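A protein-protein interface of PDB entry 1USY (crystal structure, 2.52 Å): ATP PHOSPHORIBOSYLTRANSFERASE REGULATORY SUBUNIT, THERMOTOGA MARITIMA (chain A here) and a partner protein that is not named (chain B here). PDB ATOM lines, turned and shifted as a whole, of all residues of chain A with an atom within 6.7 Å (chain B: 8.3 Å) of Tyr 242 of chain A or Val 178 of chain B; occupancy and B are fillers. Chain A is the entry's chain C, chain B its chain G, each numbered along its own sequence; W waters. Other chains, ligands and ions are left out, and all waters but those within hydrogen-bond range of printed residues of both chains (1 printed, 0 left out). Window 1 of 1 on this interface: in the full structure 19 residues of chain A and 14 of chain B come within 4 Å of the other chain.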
ATOM      1  N   GLY A 123     -20.096 -12.849 -32.353  1.00  0.00           N
ATOM      2  CA  GLY A 123     -19.538 -13.207 -31.048  1.00  0.00           C
ATOM      3  C   GLY A 123     -18.372 -12.300 -30.761  1.00  0.00           C
ATOM      4  O   GLY A 123     -17.669 -11.949 -31.722  1.00  0.00           O
ATOM      5  N   PRO A 124     -18.175 -11.933 -29.482  1.00  0.00           N
ATOM      6  CA  PRO A 124     -17.483 -10.669 -29.104  1.00  0.00           C
ATOM      7  C   PRO A 124     -16.099 -10.575 -29.725  1.00  0.00           C
ATOM      8  O   PRO A 124     -15.302 -11.516 -29.684  1.00  0.00           O
ATOM      9  CB  PRO A 124     -17.423 -10.700 -27.569  1.00  0.00           C
ATOM     10  CG  PRO A 124     -18.443 -11.741 -27.155  1.00  0.00           C
ATOM     11  CD  PRO A 124     -18.594 -12.730 -28.322  1.00  0.00           C
ATOM     12  N   VAL A 125     -15.844  -9.447 -30.361  1.00  0.00           N
ATOM     13  CA  VAL A 125     -14.664  -9.293 -31.158  1.00  0.00           C
ATOM     14  C   VAL A 125     -13.628  -8.513 -30.400  1.00  0.00           C
ATOM     15  O   VAL A 125     -13.915  -7.434 -29.806  1.00  0.00           O
ATOM     16  CB  VAL A 125     -14.981  -8.557 -32.455  1.00  0.00           C
ATOM     17  CG1 VAL A 125     -13.682  -8.180 -33.148  1.00  0.00           C
ATOM     18  CG2 VAL A 125     -15.911  -9.395 -33.355  1.00  0.00           C
ATOM     19  N   ILE A 126     -12.403  -9.026 -30.439  1.00  0.00           N
ATOM     20  CA  ILE A 126     -11.302  -8.350 -29.747  1.00  0.00           C
ATOM     21  C   ILE A 126     -10.325  -7.778 -30.749  1.00  0.00           C
ATOM     22  O   ILE A 126      -9.840  -8.489 -31.611  1.00  0.00           O
ATOM     23  CB  ILE A 126     -10.596  -9.300 -28.726  1.00  0.00           C
ATOM     24  CG1 ILE A 126     -11.610  -9.885 -27.721  1.00  0.00           C
ATOM     25  CG2 ILE A 126      -9.473  -8.596 -27.990  1.00  0.00           C
ATOM     26  CD1 ILE A 126     -11.046 -11.004 -26.884  1.00  0.00           C
ATOM     27  N   VAL A 127     -10.064  -6.475 -30.628  1.00  0.00           N
ATOM     28  CA  VAL A 127      -9.098  -5.766 -31.444  1.00  0.00           C
ATOM     29  C   VAL A 127      -7.871  -5.444 -30.566  1.00  0.00           C
ATOM     30  O   VAL A 127      -7.843  -4.464 -29.763  1.00  0.00           O
ATOM     31  CB  VAL A 127      -9.705  -4.464 -32.061  1.00  0.00           C
ATOM     32  CG1 VAL A 127      -8.660  -3.663 -32.775  1.00  0.00           C
ATOM     33  CG2 VAL A 127     -10.777  -4.783 -33.017  1.00  0.00           C
ATOM     34  N   GLU A 128      -6.844  -6.260 -30.747  1.00  0.00           N
ATOM     35  CA  GLU A 128      -5.591  -6.091 -30.010  1.00  0.00           C
ATOM     36  C   GLU A 128      -4.572  -5.187 -30.737  1.00  0.00           C
ATOM     37  O   GLU A 128      -4.213  -5.430 -31.875  1.00  0.00           O
ATOM     38  CB  GLU A 128      -5.022  -7.472 -29.676  1.00  0.00           C
ATOM     39  CG  GLU A 128      -3.648  -7.520 -29.061  1.00  0.00           C
ATOM     40  CD  GLU A 128      -3.237  -8.951 -28.778  1.00  0.00           C
ATOM     41  OE1 GLU A 128      -2.566  -9.593 -29.624  1.00  0.00           O
ATOM     42  OE2 GLU A 128      -3.631  -9.450 -27.715  1.00  0.00           O
ATOM     43  N   ARG A 187      -4.503  -4.206 -20.115  1.00  0.00           N
ATOM     44  CA  ARG A 187      -4.742  -4.196 -21.565  1.00  0.00           C
ATOM     45  C   ARG A 187      -5.705  -3.084 -21.993  1.00  0.00           C
ATOM     46  O   ARG A 187      -5.869  -2.795 -23.190  1.00  0.00           O
ATOM     47  CB  ARG A 187      -5.261  -5.565 -22.007  1.00  0.00           C
ATOM     48  CG  ARG A 187      -4.388  -6.714 -21.545  1.00  0.00           C
ATOM     49  CD  ARG A 187      -4.823  -8.176 -21.980  1.00  0.00           C
ATOM     50  NE  ARG A 187      -5.564  -8.299 -23.234  1.00  0.00           N
ATOM     51  CZ  ARG A 187      -5.031  -8.665 -24.411  1.00  0.00           C
ATOM     52  NH1 ARG A 187      -3.743  -8.928 -24.520  1.00  0.00           N
ATOM     53  NH2 ARG A 187      -5.794  -8.788 -25.489  1.00  0.00           N
ATOM     54  N   LEU A 227       4.587  -9.777 -28.784  1.00  0.00           N
ATOM     55  CA  LEU A 227       4.418  -9.969 -30.250  1.00  0.00           C
ATOM     56  C   LEU A 227       5.639  -9.388 -30.902  1.00  0.00           C
ATOM     57  O   LEU A 227       5.555  -8.720 -31.936  1.00  0.00           O
ATOM     58  CB  LEU A 227       3.159  -9.334 -30.854  1.00  0.00           C
ATOM     59  CG  LEU A 227       1.861 -10.178 -31.053  1.00  0.00           C
ATOM     60  CD1 LEU A 227       0.967 -10.097 -29.831  1.00  0.00           C
ATOM     61  CD2 LEU A 227       0.979  -9.862 -32.305  1.00  0.00           C
ATOM     62  N   THR A 240      -4.300  -7.192 -34.491  1.00  0.00           N
ATOM     63  CA  THR A 240      -4.828  -8.523 -34.751  1.00  0.00           C
ATOM     64  C   THR A 240      -6.241  -8.513 -34.217  1.00  0.00           C
ATOM     65  O   THR A 240      -6.554  -7.754 -33.296  1.00  0.00           O
ATOM     66  CB  THR A 240      -3.986  -9.645 -34.018  1.00  0.00           C
ATOM     67  OG1 THR A 240      -3.550  -9.176 -32.736  1.00  0.00           O
ATOM     68  CG2 THR A 240      -2.686  -9.890 -34.713  1.00  0.00           C
ATOM     69  N   ILE A 241      -7.103  -9.331 -34.806  1.00  0.00           N
ATOM     70  CA  ILE A 241      -8.482  -9.437 -34.365  1.00  0.00           C
ATOM     71  C   ILE A 241      -8.847 -10.887 -34.045  1.00  0.00           C
ATOM     72  O   ILE A 241      -8.533 -11.828 -34.799  1.00  0.00           O
ATOM     73  CB  ILE A 241      -9.424  -8.798 -35.416  1.00  0.00           C
ATOM     74  CG1 ILE A 241      -8.891  -7.413 -35.822  1.00  0.00           C
ATOM     75  CG2 ILE A 241     -10.811  -8.619 -34.850  1.00  0.00           C
ATOM     76  CD1 ILE A 241      -9.866  -6.504 -36.694  1.00  0.00           C
ATOM     77  N   TYR A 242      -9.520 -11.058 -32.913  1.00  0.00           N
ATOM     78  CA  TYR A 242      -9.976 -12.368 -32.470  1.00  0.00           C
ATOM     79  C   TYR A 242     -11.502 -12.460 -32.362  1.00  0.00           C
ATOM     80  O   TYR A 242     -12.156 -11.575 -31.773  1.00  0.00           O
ATOM     81  CB  TYR A 242      -9.342 -12.755 -31.129  1.00  0.00           C
ATOM     82  CG  TYR A 242      -7.832 -12.710 -31.122  1.00  0.00           C
ATOM     83  CD1 TYR A 242      -7.150 -11.535 -30.807  1.00  0.00           C
ATOM     84  CD2 TYR A 242      -7.074 -13.850 -31.393  1.00  0.00           C
ATOM     85  CE1 TYR A 242      -5.760 -11.508 -30.788  1.00  0.00           C
ATOM     86  CE2 TYR A 242      -5.653 -13.801 -31.381  1.00  0.00           C
ATOM     87  CZ  TYR A 242      -5.035 -12.635 -31.088  1.00  0.00           C
ATOM     88  OH  TYR A 242      -3.686 -12.585 -31.044  1.00  0.00           O
ATOM     89  N   ASP A 243     -12.057 -13.552 -32.884  1.00  0.00           N
ATOM     90  CA  ASP A 243     -13.476 -13.812 -32.716  1.00  0.00           C
ATOM     91  C   ASP A 243     -13.624 -14.726 -31.499  1.00  0.00           C
ATOM     92  O   ASP A 243     -13.225 -15.893 -31.562  1.00  0.00           O
ATOM     93  CB  ASP A 243     -14.070 -14.460 -33.991  1.00  0.00           C
ATOM     94  CG  ASP A 243     -15.498 -14.899 -33.805  1.00  0.00           C
ATOM     95  OD1 ASP A 243     -16.002 -15.759 -34.566  1.00  0.00           O
ATOM     96  OD2 ASP A 243     -16.212 -14.427 -32.911  1.00  0.00           O
ATOM     97  N   THR A 244     -14.171 -14.201 -30.393  1.00  0.00           N
ATOM     98  CA  THR A 244     -14.369 -15.011 -29.191  1.00  0.00           C
ATOM     99  C   THR A 244     -15.383 -16.140 -29.436  1.00  0.00           C
ATOM    100  O   THR A 244     -15.327 -17.181 -28.779  1.00  0.00           O
ATOM    101  CB  THR A 244     -14.820 -14.164 -27.986  1.00  0.00           C
ATOM    102  OG1 THR A 244     -15.899 -13.343 -28.390  1.00  0.00           O
ATOM    103  CG2 THR A 244     -13.824 -13.105 -27.632  1.00  0.00           C
ATOM    104  N   SER A 245     -16.293 -15.941 -30.392  1.00  0.00           N
ATOM    105  CA  SER A 245     -17.298 -16.960 -30.721  1.00  0.00           C
ATOM    106  C   SER A 245     -16.704 -18.292 -31.242  1.00  0.00           C
ATOM    107  O   SER A 245     -16.877 -19.327 -30.612  1.00  0.00           O
ATOM    108  CB  SER A 245     -18.367 -16.432 -31.703  1.00  0.00           C
ATOM    109  OG  SER A 245     -19.383 -17.422 -31.913  1.00  0.00           O
ATOM    110  N   SER A 246     -16.042 -18.243 -32.393  1.00  0.00           N
ATOM    111  CA  SER A 246     -15.375 -19.393 -33.001  1.00  0.00           C
ATOM    112  C   SER A 246     -13.943 -19.613 -32.514  1.00  0.00           C
ATOM    113  O   SER A 246     -13.265 -20.498 -33.018  1.00  0.00           O
ATOM    114  CB  SER A 246     -15.343 -19.241 -34.513  1.00  0.00           C
ATOM    115  OG  SER A 246     -14.572 -18.101 -34.888  1.00  0.00           O
ATOM    116  N   SER A 247     -13.509 -18.827 -31.530  1.00  0.00           N
ATOM    117  CA  SER A 247     -12.133 -18.858 -31.011  1.00  0.00           C
ATOM    118  C   SER A 247     -11.053 -18.900 -32.104  1.00  0.00           C
ATOM    119  O   SER A 247     -10.296 -19.881 -32.209  1.00  0.00           O
ATOM    120  CB  SER A 247     -11.949 -19.995 -29.981  1.00  0.00           C
ATOM    121  OG  SER A 247     -11.659 -19.467 -28.677  1.00  0.00           O
ATOM    122  N   ARG A 248     -11.037 -17.807 -33.015  1.00  0.00           N
ATOM    123  CA  ARG A 248      -9.893 -17.757 -33.944  1.00  0.00           C
ATOM    124  C   ARG A 248      -9.394 -16.317 -34.115  1.00  0.00           C
ATOM    125  O   ARG A 248     -10.097 -15.348 -33.794  1.00  0.00           O
ATOM    126  CB  ARG A 248     -10.285 -18.286 -35.326  1.00  0.00           C
ATOM    127  CG  ARG A 248     -11.736 -18.753 -35.421  1.00  0.00           C
ATOM    128  CD  ARG A 248     -12.090 -19.259 -36.816  1.00  0.00           C
ATOM    129  N   LEU A 249      -8.192 -16.308 -34.727  1.00  0.00           N
ATOM    130  CA  LEU A 249      -7.579 -15.116 -35.239  1.00  0.00           C
ATOM    131  C   LEU A 249      -8.261 -14.818 -36.577  1.00  0.00           C
ATOM    132  O   LEU A 249      -8.207 -15.577 -37.530  1.00  0.00           O
ATOM    133  CB  LEU A 249      -6.080 -15.302 -35.438  1.00  0.00           C
ATOM    134  CG  LEU A 249      -5.120 -14.109 -35.652  1.00  0.00           C
ATOM    135  CD1 LEU A 249      -3.677 -14.618 -35.759  1.00  0.00           C
ATOM    136  CD2 LEU A 249      -5.417 -13.363 -36.892  1.00  0.00           C
ATOM    137  N   VAL A 250      -8.905 -13.680 -36.640  1.00  0.00           N
ATOM    138  CA  VAL A 250      -9.768 -13.453 -37.734  1.00  0.00           C
ATOM    139  C   VAL A 250      -9.229 -12.343 -38.640  1.00  0.00           C
ATOM    140  O   VAL A 250      -9.724 -12.132 -39.727  1.00  0.00           O
ATOM    141  CB  VAL A 250     -11.147 -13.197 -37.142  1.00  0.00           C
ATOM    142  CG1 VAL A 250     -11.721 -11.818 -37.530  1.00  0.00           C
ATOM    143  CG2 VAL A 250     -12.018 -14.359 -37.472  1.00  0.00           C
ATOM    144  N   ALA A 251      -8.150 -11.690 -38.233  1.00  0.00           N
ATOM    145  CA  ALA A 251      -7.638 -10.570 -39.009  1.00  0.00           C
ATOM    146  C   ALA A 251      -6.345 -10.085 -38.420  1.00  0.00           C
ATOM    147  O   ALA A 251      -6.133 -10.162 -37.212  1.00  0.00           O
ATOM    148  CB  ALA A 251      -8.687  -9.417 -39.029  1.00  0.00           C
ATOM    149  N   LEU B  53      -3.190 -28.003 -28.920  1.00  0.00           N
ATOM    150  CA  LEU B  53      -3.164 -26.598 -28.587  1.00  0.00           C
ATOM    151  C   LEU B  53      -3.087 -25.725 -29.814  1.00  0.00           C
ATOM    152  O   LEU B  53      -3.787 -24.707 -29.894  1.00  0.00           O
ATOM    153  CB  LEU B  53      -1.960 -26.318 -27.726  1.00  0.00           C
ATOM    154  CG  LEU B  53      -2.293 -26.025 -26.272  1.00  0.00           C
ATOM    155  CD1 LEU B  53      -3.410 -26.881 -25.782  1.00  0.00           C
ATOM    156  CD2 LEU B  53      -1.095 -26.326 -25.481  1.00  0.00           C
ATOM    157  N   VAL B  54      -2.228 -26.123 -30.761  1.00  0.00           N
ATOM    158  CA  VAL B  54      -1.911 -25.310 -31.937  1.00  0.00           C
ATOM    159  C   VAL B  54      -3.142 -25.108 -32.808  1.00  0.00           C
ATOM    160  O   VAL B  54      -3.326 -24.057 -33.385  1.00  0.00           O
ATOM    161  CB  VAL B  54      -0.673 -25.897 -32.725  1.00  0.00           C
ATOM    162  CG1 VAL B  54      -0.676 -25.516 -34.200  1.00  0.00           C
ATOM    163  CG2 VAL B  54       0.651 -25.451 -32.081  1.00  0.00           C
ATOM    164  N   HIS B  55      -4.016 -26.097 -32.872  1.00  0.00           N
ATOM    165  CA  HIS B  55      -5.253 -25.962 -33.643  1.00  0.00           C
ATOM    166  C   HIS B  55      -6.352 -25.327 -32.763  1.00  0.00           C
ATOM    167  O   HIS B  55      -7.509 -25.204 -33.177  1.00  0.00           O
ATOM    168  CB  HIS B  55      -5.733 -27.319 -34.225  1.00  0.00           C
ATOM    169  CG  HIS B  55      -4.701 -28.064 -35.028  1.00  0.00           C
ATOM    170  ND1 HIS B  55      -5.041 -28.977 -36.005  1.00  0.00           N
ATOM    171  CD2 HIS B  55      -3.345 -28.047 -34.993  1.00  0.00           C
ATOM    172  CE1 HIS B  55      -3.944 -29.488 -36.536  1.00  0.00           C
ATOM    173  NE2 HIS B  55      -2.900 -28.941 -35.936  1.00  0.00           N
ATOM    174  N   GLY B  56      -5.997 -24.929 -31.549  1.00  0.00           N
ATOM    175  CA  GLY B  56      -6.977 -24.386 -30.628  1.00  0.00           C
ATOM    176  C   GLY B  56      -8.165 -25.308 -30.363  1.00  0.00           C
ATOM    177  O   GLY B  56      -9.325 -24.859 -30.329  1.00  0.00           O
ATOM    178  N   ALA B  58      -7.664 -27.448 -27.723  1.00  0.00           N
ATOM    179  CA  ALA B  58      -7.491 -27.317 -26.283  1.00  0.00           C
ATOM    180  C   ALA B  58      -6.856 -25.942 -25.981  1.00  0.00           C
ATOM    181  O   ALA B  58      -6.134 -25.448 -26.801  1.00  0.00           O
ATOM    182  CB  ALA B  58      -6.624 -28.421 -25.759  1.00  0.00           C
ATOM    183  N   ASP B  59      -7.095 -25.362 -24.800  1.00  0.00           N
ATOM    184  CA  ASP B  59      -6.545 -24.054 -24.406  1.00  0.00           C
ATOM    185  C   ASP B  59      -5.238 -24.068 -23.622  1.00  0.00           C
ATOM    186  O   ASP B  59      -4.482 -23.105 -23.666  1.00  0.00           O
ATOM    187  CB  ASP B  59      -7.568 -23.348 -23.526  1.00  0.00           C
ATOM    188  CG  ASP B  59      -8.903 -23.255 -24.186  1.00  0.00           C
ATOM    189  OD1 ASP B  59      -8.988 -22.531 -25.183  1.00  0.00           O
ATOM    190  OD2 ASP B  59      -9.899 -23.876 -23.803  1.00  0.00           O
ATOM    191  N   LEU B  75       3.844 -21.447 -28.906  1.00  0.00           N
ATOM    192  CA  LEU B  75       2.675 -20.992 -28.155  1.00  0.00           C
ATOM    193  C   LEU B  75       3.150 -20.506 -26.779  1.00  0.00           C
ATOM    194  O   LEU B  75       4.245 -20.840 -26.311  1.00  0.00           O
ATOM    195  CB  LEU B  75       1.524 -22.058 -28.036  1.00  0.00           C
ATOM    196  CG  LEU B  75       1.817 -23.511 -27.573  1.00  0.00           C
ATOM    197  CD1 LEU B  75       1.425 -24.540 -28.643  1.00  0.00           C
ATOM    198  CD2 LEU B  75       3.266 -23.830 -27.223  1.00  0.00           C
ATOM    199  N   ILE B  76       2.307 -19.712 -26.179  1.00  0.00           N
ATOM    200  CA  ILE B  76       2.590 -19.061 -24.891  1.00  0.00           C
ATOM    201  C   ILE B  76       2.944 -20.068 -23.783  1.00  0.00           C
ATOM    202  O   ILE B  76       2.381 -21.157 -23.681  1.00  0.00           O
ATOM    203  CB  ILE B  76       1.376 -18.236 -24.492  1.00  0.00           C
ATOM    204  CG1 ILE B  76       1.241 -16.990 -25.387  1.00  0.00           C
ATOM    205  CG2 ILE B  76       1.441 -17.740 -23.046  1.00  0.00           C
ATOM    206  CD1 ILE B  76      -0.199 -16.532 -25.602  1.00  0.00           C
ATOM    207  N   VAL B 175      -0.136 -22.458 -23.442  1.00  0.00           N
ATOM    208  CA  VAL B 175      -1.474 -21.926 -23.647  1.00  0.00           C
ATOM    209  C   VAL B 175      -1.630 -21.628 -25.135  1.00  0.00           C
ATOM    210  O   VAL B 175      -0.688 -21.218 -25.784  1.00  0.00           O
ATOM    211  CB  VAL B 175      -1.647 -20.633 -22.827  1.00  0.00           C
ATOM    212  CG1 VAL B 175      -3.094 -20.080 -22.938  1.00  0.00           C
ATOM    213  CG2 VAL B 175      -1.204 -20.847 -21.333  1.00  0.00           C
ATOM    214  N   ASN B 176      -2.834 -21.824 -25.659  1.00  0.00           N
ATOM    215  CA  ASN B 176      -3.142 -21.596 -27.043  1.00  0.00           C
ATOM    216  C   ASN B 176      -3.278 -20.081 -27.234  1.00  0.00           C
ATOM    217  O   ASN B 176      -4.213 -19.475 -26.712  1.00  0.00           O
ATOM    218  CB  ASN B 176      -4.442 -22.337 -27.345  1.00  0.00           C
ATOM    219  CG  ASN B 176      -5.081 -21.960 -28.700  1.00  0.00           C
ATOM    220  OD1 ASN B 176      -4.414 -21.665 -29.657  1.00  0.00           O
ATOM    221  ND2 ASN B 176      -6.397 -22.066 -28.772  1.00  0.00           N
ATOM    222  N   PRO B 177      -2.386 -19.443 -27.982  1.00  0.00           N
ATOM    223  CA  PRO B 177      -2.415 -17.983 -28.042  1.00  0.00           C
ATOM    224  C   PRO B 177      -3.801 -17.363 -28.298  1.00  0.00           C
ATOM    225  O   PRO B 177      -4.085 -16.349 -27.687  1.00  0.00           O
ATOM    226  CB  PRO B 177      -1.420 -17.630 -29.159  1.00  0.00           C
ATOM    227  CG  PRO B 177      -0.556 -18.769 -29.267  1.00  0.00           C
ATOM    228  CD  PRO B 177      -1.325 -20.015 -28.814  1.00  0.00           C
ATOM    229  N   VAL B 178      -4.649 -17.919 -29.159  1.00  0.00           N
ATOM    230  CA  VAL B 178      -5.890 -17.204 -29.395  1.00  0.00           C
ATOM    231  C   VAL B 178      -6.832 -17.294 -28.194  1.00  0.00           C
ATOM    232  O   VAL B 178      -7.500 -16.320 -27.819  1.00  0.00           O
ATOM    233  CB  VAL B 178      -6.522 -17.422 -30.801  1.00  0.00           C
ATOM    234  CG1 VAL B 178      -5.498 -17.962 -31.803  1.00  0.00           C
ATOM    235  CG2 VAL B 178      -7.775 -18.249 -30.753  1.00  0.00           C
ATOM    236  N   SER B 179      -6.865 -18.446 -27.552  1.00  0.00           N
ATOM    237  CA  SER B 179      -7.723 -18.545 -26.395  1.00  0.00           C
ATOM    238  C   SER B 179      -7.194 -17.780 -25.188  1.00  0.00           C
ATOM    239  O   SER B 179      -7.955 -17.478 -24.256  1.00  0.00           O
ATOM    240  CB  SER B 179      -8.020 -19.973 -26.054  1.00  0.00           C
ATOM    241  OG  SER B 179      -6.847 -20.717 -26.056  1.00  0.00           O
ATOM    242  N   TYR B 180      -5.908 -17.425 -25.212  1.00  0.00           N
ATOM    243  CA  TYR B 180      -5.382 -16.513 -24.201  1.00  0.00           C
ATOM    244  C   TYR B 180      -6.133 -15.228 -24.276  1.00  0.00           C
ATOM    245  O   TYR B 180      -6.240 -14.508 -23.315  1.00  0.00           O
ATOM    246  CB  TYR B 180      -3.914 -16.171 -24.377  1.00  0.00           C
ATOM    247  CG  TYR B 180      -3.196 -15.966 -23.059  1.00  0.00           C
ATOM    248  CD1 TYR B 180      -3.779 -15.235 -22.020  1.00  0.00           C
ATOM    249  CD2 TYR B 180      -1.943 -16.526 -22.839  1.00  0.00           C
ATOM    250  CE1 TYR B 180      -3.125 -15.064 -20.798  1.00  0.00           C
ATOM    251  CE2 TYR B 180      -1.276 -16.363 -21.615  1.00  0.00           C
ATOM    252  CZ  TYR B 180      -1.868 -15.630 -20.599  1.00  0.00           C
ATOM    253  OH  TYR B 180      -1.212 -15.459 -19.391  1.00  0.00           O
ATOM    254  N   ARG B 181      -6.664 -14.927 -25.429  1.00  0.00           N
ATOM    255  CA  ARG B 181      -7.322 -13.643 -25.534  1.00  0.00           C
ATOM    256  C   ARG B 181      -8.833 -13.820 -25.483  1.00  0.00           C
ATOM    257  O   ARG B 181      -9.496 -13.095 -24.742  1.00  0.00           O
ATOM    258  CB  ARG B 181      -6.809 -12.891 -26.763  1.00  0.00           C
ATOM    259  CG  ARG B 181      -5.497 -12.199 -26.450  1.00  0.00           C
ATOM    260  CD  ARG B 181      -4.463 -12.107 -27.561  1.00  0.00           C
ATOM    261  NE  ARG B 181      -3.517 -13.213 -27.501  1.00  0.00           N
ATOM    262  CZ  ARG B 181      -2.185 -13.125 -27.579  1.00  0.00           C
ATOM    263  NH1 ARG B 181      -1.517 -11.967 -27.690  1.00  0.00           N
ATOM    264  NH2 ARG B 181      -1.501 -14.238 -27.531  1.00  0.00           N
ATOM    265  N   THR B 182      -9.353 -14.845 -26.181  1.00  0.00           N
ATOM    266  CA  THR B 182     -10.809 -15.103 -26.250  1.00  0.00           C
ATOM    267  C   THR B 182     -11.396 -15.488 -24.915  1.00  0.00           C
ATOM    268  O   THR B 182     -12.562 -15.180 -24.622  1.00  0.00           O
ATOM    269  CB  THR B 182     -11.175 -16.189 -27.255  1.00  0.00           C
ATOM    270  OG1 THR B 182     -10.255 -17.287 -27.152  1.00  0.00           O
ATOM    271  CG2 THR B 182     -11.061 -15.654 -28.677  1.00  0.00           C
ATOM    272  N   LYS B 183     -10.596 -16.168 -24.112  1.00  0.00           N
ATOM    273  CA  LYS B 183     -11.064 -16.637 -22.807  1.00  0.00           C
ATOM    274  C   LYS B 183     -10.081 -16.353 -21.704  1.00  0.00           C
ATOM    275  O   LYS B 183      -9.812 -17.182 -20.860  1.00  0.00           O
ATOM    276  CB  LYS B 183     -11.421 -18.124 -22.833  1.00  0.00           C
ATOM    277  CG  LYS B 183     -10.695 -18.931 -23.794  1.00  0.00           C
ATOM    278  CD  LYS B 183     -11.651 -19.838 -24.519  1.00  0.00           C
ATOM    279  CE  LYS B 183     -11.674 -21.174 -23.885  1.00  0.00           C
ATOM    280  NZ  LYS B 183     -12.288 -22.179 -24.805  1.00  0.00           N
ATOM    281  N   ARG B 184      -9.578 -15.142 -21.713  1.00  0.00           N
ATOM    282  CA  ARG B 184      -8.519 -14.765 -20.827  1.00  0.00           C
ATOM    283  C   ARG B 184      -8.887 -14.774 -19.328  1.00  0.00           C
ATOM    284  O   ARG B 184      -8.105 -15.260 -18.507  1.00  0.00           O
ATOM    285  CB  ARG B 184      -8.009 -13.415 -21.251  1.00  0.00           C
ATOM    286  CG  ARG B 184      -8.077 -12.441 -20.163  1.00  0.00           C
ATOM    287  CD  ARG B 184      -6.912 -11.513 -20.047  1.00  0.00           C
ATOM    288  NE  ARG B 184      -7.314 -10.153 -20.369  1.00  0.00           N
ATOM    289  CZ  ARG B 184      -8.443  -9.539 -20.001  1.00  0.00           C
ATOM    290  NH1 ARG B 184      -9.351 -10.131 -19.256  1.00  0.00           N
ATOM    291  NH2 ARG B 184      -8.677  -8.288 -20.390  1.00  0.00           N
ATOM    292  N   VAL B 187      -8.571 -18.226 -18.257  1.00  0.00           N
ATOM    293  CA  VAL B 187      -7.244 -18.773 -18.399  1.00  0.00           C
ATOM    294  C   VAL B 187      -6.404 -18.254 -17.229  1.00  0.00           C
ATOM    295  O   VAL B 187      -5.790 -19.036 -16.496  1.00  0.00           O
ATOM    296  CB  VAL B 187      -6.661 -18.412 -19.814  1.00  0.00           C
ATOM    297  CG1 VAL B 187      -5.131 -18.430 -19.848  1.00  0.00           C
ATOM    298  CG2 VAL B 187      -7.254 -19.328 -20.873  1.00  0.00           C
HETATM  299  O   HOH W   1      -8.878 -21.283 -28.716  1.00  0.00           O
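The guanidinium group (NH1) of Arg 181 of chain B is in salt-bridge range of the side-chain carboxylate (OE1) of Glu 128 of chain A (3.2 Å). OG1 of Thr 182 of chain B lies within hydrogen-bond range of OG of Ser 247 of chain A.
OD2 of Asp 243 of chain A sits at hydrogen-bond distance from N of Ser 245 of chain A (2.9 Å). The guanidinium group (NE) of Arg 181 of chain B sits at hydrogen-bond distance from the backbone carbonyl oxygen (O) of Pro 177 of chain B, 3.2 Å away. The side-chain carboxylate (OD1) of Asp 243 of chain A sits at hydrogen-bond distance from the side-chain hydroxyl (OG) of Ser 246 of chain A. The backbone carbonyl oxygen of Tyr 242 of chain A sits at hydrogen-bond distance from the backbone NH of Ile 126 of chain A, at 2.9 Å. The backbone NH of Asp 243 of chain A sits at hydrogen-bond distance from the backbone carbonyl oxygen of Arg 248 of chain A (2.8 Å). OG1 of Thr 182 of chain B lies within hydrogen-bond range of O of Val 178 of chain B, at 3.0 Å.
Arg 181 of chain B touches Ile 126 of chain A. Arg 187 of chain A touches Arg 181 of chain B (NH2 to CG, 3.6 Å). Arg 184 of chain B touches Arg 187 of chain A. Arg 181 of chain B touches Leu 227 of chain A (NH1 to CD1, 3.8 Å). CB of Val 178 of chain B touches CD2 of Tyr 242 of chain A (3.7 Å). CE1 of Tyr 242 of chain A touches CD of Arg 181 of chain B (3.5 Å). Thr 182 of chain B touches Asp 243 of chain A. Thr 182 of chain B touches Thr 244 of chain A (CG2 to CA, 3.4 Å). Val 178 of chain B touches Ser 247 of chain A. Arg 248 of chain A touches Val 178 of chain B.
Of chain B, only Val 178 (3.7 Å) and Arg 181 (3.5 Å) come within 4 Å of Tyr 242 of chain A. Val 178 of chain B touches three residues of chain A. Of the printed residues of chain B, Thr 244 of chain A touches Thr 182. Of the printed residues of chain B, Arg 187 of chain A touches Arg 181 (3.6 Å) and Arg 184 (3.6 Å). Printed residues of chain B within 4 Å of Leu 227 of chain A: Arg 181. Of the printed residues of chain B, Glu 128 of chain A touches Arg 181. The nearest residue of chain B that does not touch Tyr 242 of chain A is Thr 182 of chain B (4.2 Å). The nearest printed residue of chain B that does not touch Thr 244 of chain A is Arg 181 of chain B (5.2 Å).
Hydrophobic or aromatic side chains of chain B within 4 Å of the printed part of chain A: Val 178. Along chain B the printed residues that touch a printed residue of chain A span positions 178 to 184. Hydrophobic or aromatic side chains of chain A that line the printed part of chain B: Ile 126, Leu 227 and Tyr 242.
Water W1 lies within hydrogen-bond range of ND2 of Asn 176 of chain B, OG of Ser 247 of chain A and OG of Ser 179 of chain B.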
